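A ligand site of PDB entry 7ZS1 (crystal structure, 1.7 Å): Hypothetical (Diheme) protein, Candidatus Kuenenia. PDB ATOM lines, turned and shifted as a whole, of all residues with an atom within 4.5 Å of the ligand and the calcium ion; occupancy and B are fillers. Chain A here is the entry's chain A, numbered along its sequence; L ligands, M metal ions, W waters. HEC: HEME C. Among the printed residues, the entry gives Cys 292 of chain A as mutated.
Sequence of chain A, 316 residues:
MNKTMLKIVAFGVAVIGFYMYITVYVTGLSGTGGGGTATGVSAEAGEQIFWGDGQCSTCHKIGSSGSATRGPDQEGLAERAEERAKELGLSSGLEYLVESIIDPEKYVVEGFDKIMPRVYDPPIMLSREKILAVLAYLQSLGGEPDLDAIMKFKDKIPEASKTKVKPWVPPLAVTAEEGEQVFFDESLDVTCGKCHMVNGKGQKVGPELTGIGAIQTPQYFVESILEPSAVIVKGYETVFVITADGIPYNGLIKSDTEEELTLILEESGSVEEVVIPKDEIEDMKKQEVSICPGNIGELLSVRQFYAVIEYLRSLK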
ATOM      1  N   ARG A  70      30.390  -6.399 -25.609  1.00  0.00           N
ATOM      2  CA  ARG A  70      29.890  -5.693 -24.423  1.00  0.00           C
ATOM      3  C   ARG A  70      30.310  -6.381 -23.133  1.00  0.00           C
ATOM      4  O   ARG A  70      30.530  -5.717 -22.115  1.00  0.00           O
ATOM      5  CB  ARG A  70      28.362  -5.593 -24.459  1.00  0.00           C
ATOM      6  CG  ARG A  70      27.753  -5.038 -25.750  1.00  0.00           C
ATOM      7  CD  ARG A  70      27.998  -3.539 -25.937  1.00  0.00           C
ATOM      8  NE  ARG A  70      28.248  -3.190 -27.340  1.00  0.00           N
ATOM      9  CZ  ARG A  70      27.351  -2.655 -28.169  1.00  0.00           C
ATOM     10  NH1 ARG A  70      26.123  -2.377 -27.754  1.00  0.00           N
ATOM     11  NH2 ARG A  70      27.686  -2.383 -29.423  1.00  0.00           N
ATOM     12  N   ILE A 115      26.548  -3.726 -16.464  1.00  0.00           N
ATOM     13  CA  ILE A 115      25.612  -3.626 -17.569  1.00  0.00           C
ATOM     14  C   ILE A 115      24.751  -4.876 -17.730  1.00  0.00           C
ATOM     15  O   ILE A 115      23.668  -4.800 -18.336  1.00  0.00           O
ATOM     16  CB  ILE A 115      26.346  -3.297 -18.889  1.00  0.00           C
ATOM     17  CG1 ILE A 115      25.379  -2.894 -20.008  1.00  0.00           C
ATOM     18  CG2 ILE A 115      27.196  -4.477 -19.325  1.00  0.00           C
ATOM     19  CD1 ILE A 115      26.090  -2.198 -21.207  1.00  0.00           C
ATOM     20  N   VAL A 190      19.821  18.658 -27.280  1.00  0.00           N
ATOM     21  CA  VAL A 190      20.454  17.346 -27.379  1.00  0.00           C
ATOM     22  C   VAL A 190      19.643  16.526 -28.377  1.00  0.00           C
ATOM     23  O   VAL A 190      18.409  16.573 -28.362  1.00  0.00           O
ATOM     24  CB  VAL A 190      20.561  16.633 -26.004  1.00  0.00           C
ATOM     25  CG1 VAL A 190      19.192  16.306 -25.443  1.00  0.00           C
ATOM     26  CG2 VAL A 190      21.430  15.380 -26.107  1.00  0.00           C
ATOM     27  N   THR A 191      20.341  15.779 -29.234  1.00  0.00           N
ATOM     28  CA  THR A 191      19.710  14.935 -30.247  1.00  0.00           C
ATOM     29  C   THR A 191      20.347  13.554 -30.194  1.00  0.00           C
ATOM     30  O   THR A 191      21.474  13.377 -30.653  1.00  0.00           O
ATOM     31  CB  THR A 191      19.884  15.520 -31.652  1.00  0.00           C
ATOM     32  OG1 THR A 191      19.457  16.888 -31.659  1.00  0.00           O
ATOM     33  CG2 THR A 191      19.110  14.678 -32.652  1.00  0.00           C
ATOM     34  N   CYS A 192      19.622  12.559 -29.662  1.00  0.00           N
ATOM     35  CA  CYS A 192      20.217  11.228 -29.529  1.00  0.00           C
ATOM     36  C   CYS A 192      20.679  10.679 -30.873  1.00  0.00           C
ATOM     37  O   CYS A 192      21.723  10.013 -30.957  1.00  0.00           O
ATOM     38  CB  CYS A 192      19.226  10.238 -28.889  1.00  0.00           C
ATOM     39  SG  CYS A 192      18.315  10.896 -27.484  1.00  0.00           S
ATOM     40  N   CYS A 195      24.251  10.649 -32.392  1.00  0.00           N
ATOM     41  CA  CYS A 195      25.266   9.675 -31.997  1.00  0.00           C
ATOM     42  C   CYS A 195      24.803   8.237 -32.042  1.00  0.00           C
ATOM     43  O   CYS A 195      25.647   7.335 -32.047  1.00  0.00           O
ATOM     44  CB  CYS A 195      25.772   9.973 -30.579  1.00  0.00           C
ATOM     45  SG  CYS A 195      26.694  11.528 -30.454  1.00  0.00           S
ATOM     46  N   HIS A 196      23.502   7.981 -32.098  1.00  0.00           N
ATOM     47  CA  HIS A 196      22.955   6.649 -31.976  1.00  0.00           C
ATOM     48  C   HIS A 196      22.109   6.306 -33.185  1.00  0.00           C
ATOM     49  O   HIS A 196      21.263   7.097 -33.598  1.00  0.00           O
ATOM     50  CB  HIS A 196      22.086   6.511 -30.741  1.00  0.00           C
ATOM     51  CG  HIS A 196      22.855   6.465 -29.462  1.00  0.00           C
ATOM     52  ND1 HIS A 196      23.626   5.383 -29.103  1.00  0.00           N
ATOM     53  CD2 HIS A 196      22.944   7.346 -28.452  1.00  0.00           C
ATOM     54  CE1 HIS A 196      24.174   5.607 -27.929  1.00  0.00           C
ATOM     55  NE2 HIS A 196      23.763   6.786 -27.503  1.00  0.00           N
ATOM     56  N   VAL A 205      28.064   7.117 -33.657  1.00  0.00           N
ATOM     57  CA  VAL A 205      29.133   7.574 -32.774  1.00  0.00           C
ATOM     58  C   VAL A 205      29.151   6.649 -31.562  1.00  0.00           C
ATOM     59  O   VAL A 205      30.156   5.980 -31.281  1.00  0.00           O
ATOM     60  CB  VAL A 205      28.917   9.029 -32.332  1.00  0.00           C
ATOM     61  CG1 VAL A 205      29.947   9.456 -31.305  1.00  0.00           C
ATOM     62  CG2 VAL A 205      28.934   9.974 -33.560  1.00  0.00           C
ATOM     63  N   GLY A 206      28.037   6.601 -30.851  1.00  0.00           N
ATOM     64  CA  GLY A 206      27.847   5.638 -29.797  1.00  0.00           C
ATOM     65  C   GLY A 206      27.263   4.356 -30.338  1.00  0.00           C
ATOM     66  O   GLY A 206      27.028   4.219 -31.542  1.00  0.00           O
ATOM     67  N   PRO A 207      27.005   3.389 -29.455  1.00  0.00           N
ATOM     68  CA  PRO A 207      26.458   2.097 -29.909  1.00  0.00           C
ATOM     69  C   PRO A 207      25.093   2.239 -30.577  1.00  0.00           C
ATOM     70  O   PRO A 207      24.258   3.068 -30.202  1.00  0.00           O
ATOM     71  CB  PRO A 207      26.353   1.279 -28.612  1.00  0.00           C
ATOM     72  CG  PRO A 207      26.452   2.277 -27.499  1.00  0.00           C
ATOM     73  CD  PRO A 207      27.284   3.409 -28.012  1.00  0.00           C
ATOM     74  N   LEU A 209      21.396   1.352 -31.060  1.00  0.00           N
ATOM     75  CA  LEU A 209      20.416   0.986 -30.036  1.00  0.00           C
ATOM     76  C   LEU A 209      19.304   0.083 -30.541  1.00  0.00           C
ATOM     77  O   LEU A 209      18.462  -0.334 -29.749  1.00  0.00           O
ATOM     78  CB  LEU A 209      19.804   2.257 -29.409  1.00  0.00           C
ATOM     79  CG  LEU A 209      20.829   3.196 -28.750  1.00  0.00           C
ATOM     80  CD1 LEU A 209      20.169   4.383 -28.064  1.00  0.00           C
ATOM     81  CD2 LEU A 209      21.715   2.416 -27.725  1.00  0.00           C
ATOM     82  N   ILE A 212      17.522  -2.699 -28.267  1.00  0.00           N
ATOM     83  CA  ILE A 212      17.942  -2.639 -26.865  1.00  0.00           C
ATOM     84  C   ILE A 212      16.753  -2.781 -25.917  1.00  0.00           C
ATOM     85  O   ILE A 212      16.922  -3.201 -24.763  1.00  0.00           O
ATOM     86  CB  ILE A 212      18.718  -1.345 -26.591  1.00  0.00           C
ATOM     87  CG1 ILE A 212      19.442  -1.456 -25.241  1.00  0.00           C
ATOM     88  CG2 ILE A 212      17.793  -0.128 -26.615  1.00  0.00           C
ATOM     89  CD1 ILE A 212      20.472  -0.316 -24.954  1.00  0.00           C
ATOM     90  N   TYR A 220      17.807   1.058 -16.429  1.00  0.00           N
ATOM     91  CA  TYR A 220      19.076   1.219 -17.123  1.00  0.00           C
ATOM     92  C   TYR A 220      19.030   2.395 -18.099  1.00  0.00           C
ATOM     93  O   TYR A 220      20.003   3.136 -18.240  1.00  0.00           O
ATOM     94  CB  TYR A 220      19.434  -0.061 -17.860  1.00  0.00           C
ATOM     95  CG  TYR A 220      20.715   0.101 -18.640  1.00  0.00           C
ATOM     96  CD1 TYR A 220      21.943   0.150 -17.986  1.00  0.00           C
ATOM     97  CD2 TYR A 220      20.709   0.181 -20.032  1.00  0.00           C
ATOM     98  CE1 TYR A 220      23.138   0.292 -18.695  1.00  0.00           C
ATOM     99  CE2 TYR A 220      21.905   0.331 -20.747  1.00  0.00           C
ATOM    100  CZ  TYR A 220      23.104   0.388 -20.072  1.00  0.00           C
ATOM    101  OH  TYR A 220      24.277   0.523 -20.798  1.00  0.00           O
ATOM    102  N   PHE A 221      17.897   2.571 -18.788  1.00  0.00           N
ATOM    103  CA  PHE A 221      17.803   3.719 -19.693  1.00  0.00           C
ATOM    104  C   PHE A 221      17.858   5.029 -18.911  1.00  0.00           C
ATOM    105  O   PHE A 221      18.540   5.978 -19.325  1.00  0.00           O
ATOM    106  CB  PHE A 221      16.547   3.660 -20.553  1.00  0.00           C
ATOM    107  CG  PHE A 221      16.414   2.413 -21.392  1.00  0.00           C
ATOM    108  CD1 PHE A 221      17.519   1.846 -22.002  1.00  0.00           C
ATOM    109  CD2 PHE A 221      15.170   1.814 -21.578  1.00  0.00           C
ATOM    110  CE1 PHE A 221      17.401   0.689 -22.758  1.00  0.00           C
ATOM    111  CE2 PHE A 221      15.036   0.672 -22.354  1.00  0.00           C
ATOM    112  CZ  PHE A 221      16.151   0.106 -22.941  1.00  0.00           C
ATOM    113  N   SER A 224      21.411   5.534 -17.985  1.00  0.00           N
ATOM    114  CA  SER A 224      22.251   5.846 -19.151  1.00  0.00           C
ATOM    115  C   SER A 224      22.136   7.309 -19.539  1.00  0.00           C
ATOM    116  O   SER A 224      23.140   7.921 -19.936  1.00  0.00           O
ATOM    117  CB  SER A 224      21.862   4.974 -20.350  1.00  0.00           C
ATOM    118  OG  SER A 224      22.153   3.619 -20.074  1.00  0.00           O
ATOM    119  N   ILE A 225      20.934   7.898 -19.437  1.00  0.00           N
ATOM    120  CA  ILE A 225      20.669   9.263 -19.890  1.00  0.00           C
ATOM    121  C   ILE A 225      21.110  10.282 -18.839  1.00  0.00           C
ATOM    122  O   ILE A 225      21.631  11.355 -19.173  1.00  0.00           O
ATOM    123  CB  ILE A 225      19.169   9.427 -20.222  1.00  0.00           C
ATOM    124  CG1 ILE A 225      18.778   8.543 -21.402  1.00  0.00           C
ATOM    125  CG2 ILE A 225      18.815  10.879 -20.482  1.00  0.00           C
ATOM    126  CD1 ILE A 225      17.248   8.358 -21.588  1.00  0.00           C
ATOM    127  N   PRO A 228      25.468   9.204 -17.542  1.00  0.00           N
ATOM    128  CA  PRO A 228      26.060   8.505 -18.707  1.00  0.00           C
ATOM    129  C   PRO A 228      27.405   7.855 -18.438  1.00  0.00           C
ATOM    130  O   PRO A 228      27.719   6.832 -19.062  1.00  0.00           O
ATOM    131  CB  PRO A 228      26.186   9.614 -19.765  1.00  0.00           C
ATOM    132  CG  PRO A 228      26.060  10.937 -18.984  1.00  0.00           C
ATOM    133  CD  PRO A 228      25.115  10.603 -17.864  1.00  0.00           C
ATOM    134  N   VAL A 231      28.019   3.805 -16.286  1.00  0.00           N
ATOM    135  CA  VAL A 231      28.311   2.560 -16.991  1.00  0.00           C
ATOM    136  C   VAL A 231      28.803   2.947 -18.373  1.00  0.00           C
ATOM    137  O   VAL A 231      28.170   3.757 -19.037  1.00  0.00           O
ATOM    138  CB  VAL A 231      27.061   1.671 -17.119  1.00  0.00           C
ATOM    139  CG1 VAL A 231      27.311   0.543 -18.136  1.00  0.00           C
ATOM    140  CG2 VAL A 231      26.677   1.099 -15.797  1.00  0.00           C
ATOM    141  N   ILE A 232      29.924   2.375 -18.802  1.00  0.00           N
ATOM    142  CA  ILE A 232      30.486   2.717 -20.101  1.00  0.00           C
ATOM    143  C   ILE A 232      30.523   1.451 -20.934  1.00  0.00           C
ATOM    144  O   ILE A 232      31.226   0.491 -20.599  1.00  0.00           O
ATOM    145  CB  ILE A 232      31.872   3.357 -19.993  1.00  0.00           C
ATOM    146  CG1 ILE A 232      31.736   4.681 -19.211  1.00  0.00           C
ATOM    147  CG2 ILE A 232      32.463   3.623 -21.378  1.00  0.00           C
ATOM    148  CD1 ILE A 232      33.047   5.414 -19.024  1.00  0.00           C
ATOM    149  N   VAL A 233      29.728   1.437 -22.003  1.00  0.00           N
ATOM    150  CA  VAL A 233      29.760   0.300 -22.919  1.00  0.00           C
ATOM    151  C   VAL A 233      31.194   0.029 -23.349  1.00  0.00           C
ATOM    152  O   VAL A 233      31.918   0.928 -23.771  1.00  0.00           O
ATOM    153  CB  VAL A 233      28.852   0.579 -24.131  1.00  0.00           C
ATOM    154  CG1 VAL A 233      28.944  -0.575 -25.127  1.00  0.00           C
ATOM    155  CG2 VAL A 233      27.367   0.854 -23.675  1.00  0.00           C
ATOM    156  N   TYR A 236      33.785   1.967 -25.865  1.00  0.00           N
ATOM    157  CA  TYR A 236      33.376   3.353 -26.077  1.00  0.00           C
ATOM    158  C   TYR A 236      33.931   4.279 -25.002  1.00  0.00           C
ATOM    159  O   TYR A 236      33.341   5.313 -24.702  1.00  0.00           O
ATOM    160  CB  TYR A 236      31.857   3.448 -26.135  1.00  0.00           C
ATOM    161  CG  TYR A 236      31.289   2.799 -27.366  1.00  0.00           C
ATOM    162  CD1 TYR A 236      31.012   1.426 -27.402  1.00  0.00           C
ATOM    163  CD2 TYR A 236      31.000   3.551 -28.483  1.00  0.00           C
ATOM    164  CE1 TYR A 236      30.475   0.842 -28.546  1.00  0.00           C
ATOM    165  CE2 TYR A 236      30.455   2.980 -29.611  1.00  0.00           C
ATOM    166  CZ  TYR A 236      30.214   1.636 -29.646  1.00  0.00           C
ATOM    167  OH  TYR A 236      29.676   1.098 -30.796  1.00  0.00           O
ATOM    168  N   LEU A 252      36.415   9.808 -28.466  1.00  0.00           N
ATOM    169  CA  LEU A 252      36.137   8.405 -28.710  1.00  0.00           C
ATOM    170  C   LEU A 252      36.886   7.928 -29.951  1.00  0.00           C
ATOM    171  O   LEU A 252      36.897   8.609 -30.971  1.00  0.00           O
ATOM    172  CB  LEU A 252      34.622   8.246 -28.890  1.00  0.00           C
ATOM    173  CG  LEU A 252      34.019   6.928 -29.346  1.00  0.00           C
ATOM    174  CD1 LEU A 252      34.163   5.907 -28.218  1.00  0.00           C
ATOM    175  CD2 LEU A 252      32.552   7.153 -29.685  1.00  0.00           C
ATOM    176  N   GLU A 266      33.750  15.598 -28.468  1.00  0.00           N
ATOM    177  CA  GLU A 266      32.405  16.004 -28.100  1.00  0.00           C
ATOM    178  C   GLU A 266      32.485  17.290 -27.292  1.00  0.00           C
ATOM    179  O   GLU A 266      33.422  17.476 -26.506  1.00  0.00           O
ATOM    180  CB  GLU A 266      31.668  14.920 -27.305  1.00  0.00           C
ATOM    181  CG  GLU A 266      30.225  15.297 -26.919  1.00  0.00           C
ATOM    182  CD  GLU A 266      30.171  16.154 -25.662  1.00  0.00           C
ATOM    183  OE1 GLU A 266      31.102  16.053 -24.832  1.00  0.00           O
ATOM    184  OE2 GLU A 266      29.198  16.930 -25.502  1.00  0.00           O
ATOM    185  N   GLY A 269      27.146  18.529 -26.506  1.00  0.00           N
ATOM    186  CA  GLY A 269      26.347  17.678 -27.365  1.00  0.00           C
ATOM    187  C   GLY A 269      26.726  17.686 -28.836  1.00  0.00           C
ATOM    188  O   GLY A 269      26.194  16.858 -29.595  1.00  0.00           O
ATOM    189  N   VAL A 271      29.555  17.168 -31.946  1.00  0.00           N
ATOM    190  CA  VAL A 271      30.680  16.275 -32.179  1.00  0.00           C
ATOM    191  C   VAL A 271      31.508  16.790 -33.356  1.00  0.00           C
ATOM    192  O   VAL A 271      31.013  17.555 -34.209  1.00  0.00           O
ATOM    193  CB  VAL A 271      30.229  14.819 -32.429  1.00  0.00           C
ATOM    194  CG1 VAL A 271      29.779  14.167 -31.119  1.00  0.00           C
ATOM    195  CG2 VAL A 271      29.102  14.781 -33.435  1.00  0.00           C
ATOM    196  N   SER A 290      32.453   8.954 -20.547  1.00  0.00           N
ATOM    197  CA  SER A 290      31.683   8.791 -21.773  1.00  0.00           C
ATOM    198  C   SER A 290      31.471  10.142 -22.450  1.00  0.00           C
ATOM    199  O   SER A 290      31.391  11.168 -21.768  1.00  0.00           O
ATOM    200  CB  SER A 290      30.305   8.182 -21.471  1.00  0.00           C
ATOM    201  OG  SER A 290      29.536   7.979 -22.647  1.00  0.00           O
ATOM    202  N   ILE A 291      31.324  10.130 -23.768  1.00  0.00           N
ATOM    203  CA  ILE A 291      30.850  11.339 -24.445  1.00  0.00           C
ATOM    204  C   ILE A 291      29.323  11.385 -24.578  1.00  0.00           C
ATOM    205  O   ILE A 291      28.787  12.402 -25.051  1.00  0.00           O
ATOM    206  CB  ILE A 291      31.520  11.544 -25.823  1.00  0.00           C
ATOM    207  CG1 ILE A 291      31.122  10.438 -26.809  1.00  0.00           C
ATOM    208  CG2 ILE A 291      33.027  11.714 -25.649  1.00  0.00           C
ATOM    209  CD1 ILE A 291      31.553  10.763 -28.300  1.00  0.00           C
ATOM    210  N   CYS A 292      28.592  10.346 -24.148  1.00  0.00           N
ATOM    211  CA  CYS A 292      27.137  10.479 -23.985  1.00  0.00           C
ATOM    212  C   CYS A 292      26.892  11.682 -23.054  1.00  0.00           C
ATOM    213  O   CYS A 292      27.436  11.715 -21.946  1.00  0.00           O
ATOM    214  CB  CYS A 292      26.554   9.173 -23.397  1.00  0.00           C
ATOM    215  SG  CYS A 292      24.742   8.896 -23.590  1.00  0.00           S
ATOM    216  N   PRO A 293      26.156  12.718 -23.506  1.00  0.00           N
ATOM    217  CA  PRO A 293      26.309  14.046 -22.866  1.00  0.00           C
ATOM    218  C   PRO A 293      25.872  14.053 -21.411  1.00  0.00           C
ATOM    219  O   PRO A 293      24.895  13.421 -21.016  1.00  0.00           O
ATOM    220  CB  PRO A 293      25.415  14.962 -23.727  1.00  0.00           C
ATOM    221  CG  PRO A 293      25.329  14.269 -25.040  1.00  0.00           C
ATOM    222  CD  PRO A 293      25.371  12.790 -24.752  1.00  0.00           C
ATOM    223  N   ILE A 296      22.012  15.908 -19.888  1.00  0.00           N
ATOM    224  CA  ILE A 296      20.760  15.629 -20.581  1.00  0.00           C
ATOM    225  C   ILE A 296      19.590  15.999 -19.668  1.00  0.00           C
ATOM    226  O   ILE A 296      18.570  16.519 -20.139  1.00  0.00           O
ATOM    227  CB  ILE A 296      20.678  14.162 -21.042  1.00  0.00           C
ATOM    228  CG1 ILE A 296      21.731  13.904 -22.135  1.00  0.00           C
ATOM    229  CG2 ILE A 296      19.312  13.880 -21.649  1.00  0.00           C
ATOM    230  CD1 ILE A 296      21.931  12.431 -22.480  1.00  0.00           C
ATOM    231  N   LEU A 300      16.443  18.217 -21.511  1.00  0.00           N
ATOM    232  CA  LEU A 300      15.157  17.641 -21.875  1.00  0.00           C
ATOM    233  C   LEU A 300      14.136  18.009 -20.809  1.00  0.00           C
ATOM    234  O   LEU A 300      14.449  18.074 -19.615  1.00  0.00           O
ATOM    235  CB  LEU A 300      15.270  16.114 -21.983  1.00  0.00           C
ATOM    236  CG  LEU A 300      16.119  15.537 -23.122  1.00  0.00           C
ATOM    237  CD1 LEU A 300      16.019  14.028 -23.124  1.00  0.00           C
ATOM    238  CD2 LEU A 300      15.672  16.129 -24.454  1.00  0.00           C
ATOM    239  N   VAL A 308      11.285   9.612 -24.411  1.00  0.00           N
ATOM    240  CA  VAL A 308      12.453   8.950 -24.978  1.00  0.00           C
ATOM    241  C   VAL A 308      12.619   7.570 -24.360  1.00  0.00           C
ATOM    242  O   VAL A 308      12.953   6.590 -25.040  1.00  0.00           O
ATOM    243  CB  VAL A 308      13.717   9.814 -24.774  1.00  0.00           C
ATOM    244  CG1 VAL A 308      14.967   9.028 -25.137  1.00  0.00           C
ATOM    245  CG2 VAL A 308      13.624  11.134 -25.587  1.00  0.00           C
ATOM    246  N   LEU A 312      12.866   3.913 -26.282  1.00  0.00           N
ATOM    247  CA  LEU A 312      13.883   2.878 -26.087  1.00  0.00           C
ATOM    248  C   LEU A 312      13.249   1.544 -25.703  1.00  0.00           C
ATOM    249  O   LEU A 312      13.645   0.487 -26.207  1.00  0.00           O
ATOM    250  CB  LEU A 312      14.885   3.324 -25.022  1.00  0.00           C
ATOM    251  CG  LEU A 312      15.740   4.539 -25.387  1.00  0.00           C
ATOM    252  CD1 LEU A 312      16.535   4.982 -24.191  1.00  0.00           C
ATOM    253  CD2 LEU A 312      16.698   4.207 -26.530  1.00  0.00           C
HETATM  254 FE   HEC L   1      24.128   7.872 -25.649  1.00  0.00          FE
HETATM  255  CHA HEC L   1      25.594   4.950 -24.537  1.00  0.00           C
HETATM  256  CHB HEC L   1      21.090   6.721 -24.592  1.00  0.00           C
HETATM  257  CHC HEC L   1      22.656  10.702 -26.844  1.00  0.00           C
HETATM  258  CHD HEC L   1      27.096   8.826 -27.145  1.00  0.00           C
HETATM  259  NA  HEC L   1      23.492   6.170 -24.702  1.00  0.00           N
HETATM  260  C1A HEC L   1      24.238   5.063 -24.408  1.00  0.00           C
HETATM  261  C2A HEC L   1      23.344   4.033 -23.907  1.00  0.00           C
HETATM  262  C3A HEC L   1      22.097   4.533 -23.933  1.00  0.00           C
HETATM  263  C4A HEC L   1      22.175   5.874 -24.442  1.00  0.00           C
HETATM  264  CMA HEC L   1      20.795   3.803 -23.513  1.00  0.00           C
HETATM  265  CAA HEC L   1      23.784   2.623 -23.466  1.00  0.00           C
HETATM  266  CBA HEC L   1      23.798   1.768 -24.732  1.00  0.00           C
HETATM  267  CGA HEC L   1      24.025   0.296 -24.433  1.00  0.00           C
HETATM  268  O1A HEC L   1      24.260  -0.437 -25.430  1.00  0.00           O
HETATM  269  O2A HEC L   1      24.010  -0.172 -23.241  1.00  0.00           O
HETATM  270  NB  HEC L   1      22.256   8.561 -25.696  1.00  0.00           N
HETATM  271  C1B HEC L   1      21.130   7.966 -25.167  1.00  0.00           C
HETATM  272  C2B HEC L   1      20.017   8.883 -25.275  1.00  0.00           C
HETATM  273  C3B HEC L   1      20.437   9.978 -25.936  1.00  0.00           C
HETATM  274  C4B HEC L   1      21.846   9.807 -26.189  1.00  0.00           C
HETATM  275  CMB HEC L   1      18.569   8.560 -24.841  1.00  0.00           C
HETATM  276  CAB HEC L   1      19.608  11.223 -26.324  1.00  0.00           C
HETATM  277  CBB HEC L   1      18.958  11.846 -25.055  1.00  0.00           C
HETATM  278  NC  HEC L   1      24.772   9.431 -26.803  1.00  0.00           N
HETATM  279  C1C HEC L   1      23.979  10.505 -27.143  1.00  0.00           C
HETATM  280  C2C HEC L   1      24.824  11.475 -27.804  1.00  0.00           C
HETATM  281  C3C HEC L   1      26.035  10.975 -27.989  1.00  0.00           C
HETATM  282  C4C HEC L   1      26.032   9.678 -27.300  1.00  0.00           C
HETATM  283  CMC HEC L   1      24.243  12.772 -28.419  1.00  0.00           C
HETATM  284  CAC HEC L   1      27.213  11.660 -28.751  1.00  0.00           C
HETATM  285  CBC HEC L   1      27.654  12.998 -28.134  1.00  0.00           C
HETATM  286  ND  HEC L   1      26.004   7.022 -25.820  1.00  0.00           N
HETATM  287  C1D HEC L   1      27.095   7.641 -26.434  1.00  0.00           C
HETATM  288  C2D HEC L   1      28.271   6.841 -26.241  1.00  0.00           C
HETATM  289  C3D HEC L   1      27.825   5.632 -25.431  1.00  0.00           C
HETATM  290  C4D HEC L   1      26.413   5.834 -25.222  1.00  0.00           C
HETATM  291  CMD HEC L   1      29.703   7.130 -26.748  1.00  0.00           C
HETATM  292  CAD HEC L   1      28.730   4.473 -24.964  1.00  0.00           C
HETATM  293  CBD HEC L   1      29.410   4.813 -23.628  1.00  0.00           C
HETATM  294  CGD HEC L   1      28.414   4.845 -22.490  1.00  0.00           C
HETATM  295  O1D HEC L   1      28.132   5.965 -21.967  1.00  0.00           O
HETATM  296  O2D HEC L   1      27.889   3.761 -22.100  1.00  0.00           O
HETATM  297 CA    CA M   1      26.701   5.033 -20.252  1.00  0.00          CA
HETATM  298  O   HOH W   1      25.015   3.270 -20.304  1.00  0.00           O
HETATM  299  O   HOH W   2      25.532   5.126 -18.057  1.00  0.00           O
HETATM  300  O   HOH W   3      24.966   6.478 -21.261  1.00  0.00           O
HETATM  301  O   HOH W   4      23.235  -1.145 -27.784  1.00  0.00           O
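A carbon (CAB) of the ligand is bonded to the side-chain sulfur of Cys 192 (1.8 Å).
A carbon (CAC) of the ligand is bonded to the side-chain sulfur (SG) of Cys 195 (1.8 Å).
FE of the ligand is bound by NE2 of His 196.
SG of Cys 292 is bound to FE of the ligand, 2.4 Å away.
O1D of the ligand sits close to OG of Ser 290.
OH of Tyr 220 sits at hydrogen-bond distance from O2A of the ligand.
The backbone NH of Val 233 sits close to an oxygen (O2D) of the ligand, at 3.0 Å.
The guanidinium group (NH1) of Arg 70 lies within salt-bridge range of an oxygen (O1A) of the ligand (3.6 Å).
The backbone NH (N) of Gly 206 lies within hydrogen-bond range of the backbone carbonyl oxygen (O) of Cys 195 (2.8 Å).
The backbone NH (N) of Val 205 sits at hydrogen-bond distance from the backbone carbonyl oxygen (O) of Cys 195 (2.9 Å).
O of Pro 207 lies within hydrogen-bond range of ND1 of His 196, at 2.6 Å.
The backbone NH of Cys 292 is in hydrogen-bond range of the side-chain hydroxyl of Ser 290 (3.0 Å).
OG of Ser 224 sits at hydrogen-bond distance from O of Tyr 220, 2.9 Å away.
OE2 of Glu 266 sits at hydrogen-bond distance from N of Gly 269.
Ile 115 touches the ligand.
Thr 191 touches the ligand.
Gly 206 touches the ligand.
Pro 207 touches the ligand (CD to C3D, 3.4 Å).
CD2 of Leu 209 touches CBA of the ligand, 3.7 Å away.
CD1 of Ile 212 touches CGA of the ligand, 3.6 Å away.
Ser 224 touches the ligand (CB to CMA, 3.5 Å).
Ile 225 touches the ligand.
CA of Ile 232 touches O2D of the ligand, 3.4 Å away.
CB of Tyr 236 touches CAD of the ligand, at 3.5 Å.
CG of Glu 266 touches CBC of the ligand, 3.7 Å away.
Val 271 touches the ligand (CG1 to CBC, 3.8 Å).
Ile 291 touches the ligand.
Pro 293 touches the ligand.
Ile 296 touches the ligand (CD1 to CBB, 3.98 Å).
Val 308 touches the ligand (CG1 to CMB, 3.6 Å).
26 residues have an atom within 4 Å of the ligand: Arg 70, Ile 115, Thr 191, Cys 192, Cys 195, His 196, Gly 206, Pro 207, Leu 209, Ile 212, Tyr 220, Ser 224, Ile 225, Pro 228, Val 231, Ile 232, Val 233, Tyr 236, Glu 266, Val 271, Ser 290, Ile 291, Cys 292, Pro 293, Ile 296 and Val 308.
The nearest printed residue that does not touch the ligand is Leu 252 (4.1 Å).
Of the 33 residues printed, 2 come within 4 Å of the calcium ion.
The nearest printed residue that does not touch the calcium ion is Ile 232 (4.4 Å).
The backbone carbonyl oxygen (O) of Val 231 binds the calcium ion (2.3 Å).
The calcium ion is bound by O of Pro 228, at 2.4 Å.
The calcium ion is bound by an oxygen (O1D) of the ligand (2.4 Å).
Water W1 is bound to the calcium ion, 2.4 Å away.
Water W3 is bound to the calcium ion.
The calcium ion is bound by water W2 (2.5 Å).
The calcium ion is bound by O2D of the ligand.
Water W1 bridges OH of Tyr 220 and OG of Ser 224.
Water W4 bridges O1A of the ligand (2.7 Å) and NH1 of Arg 70 (3.1 Å).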
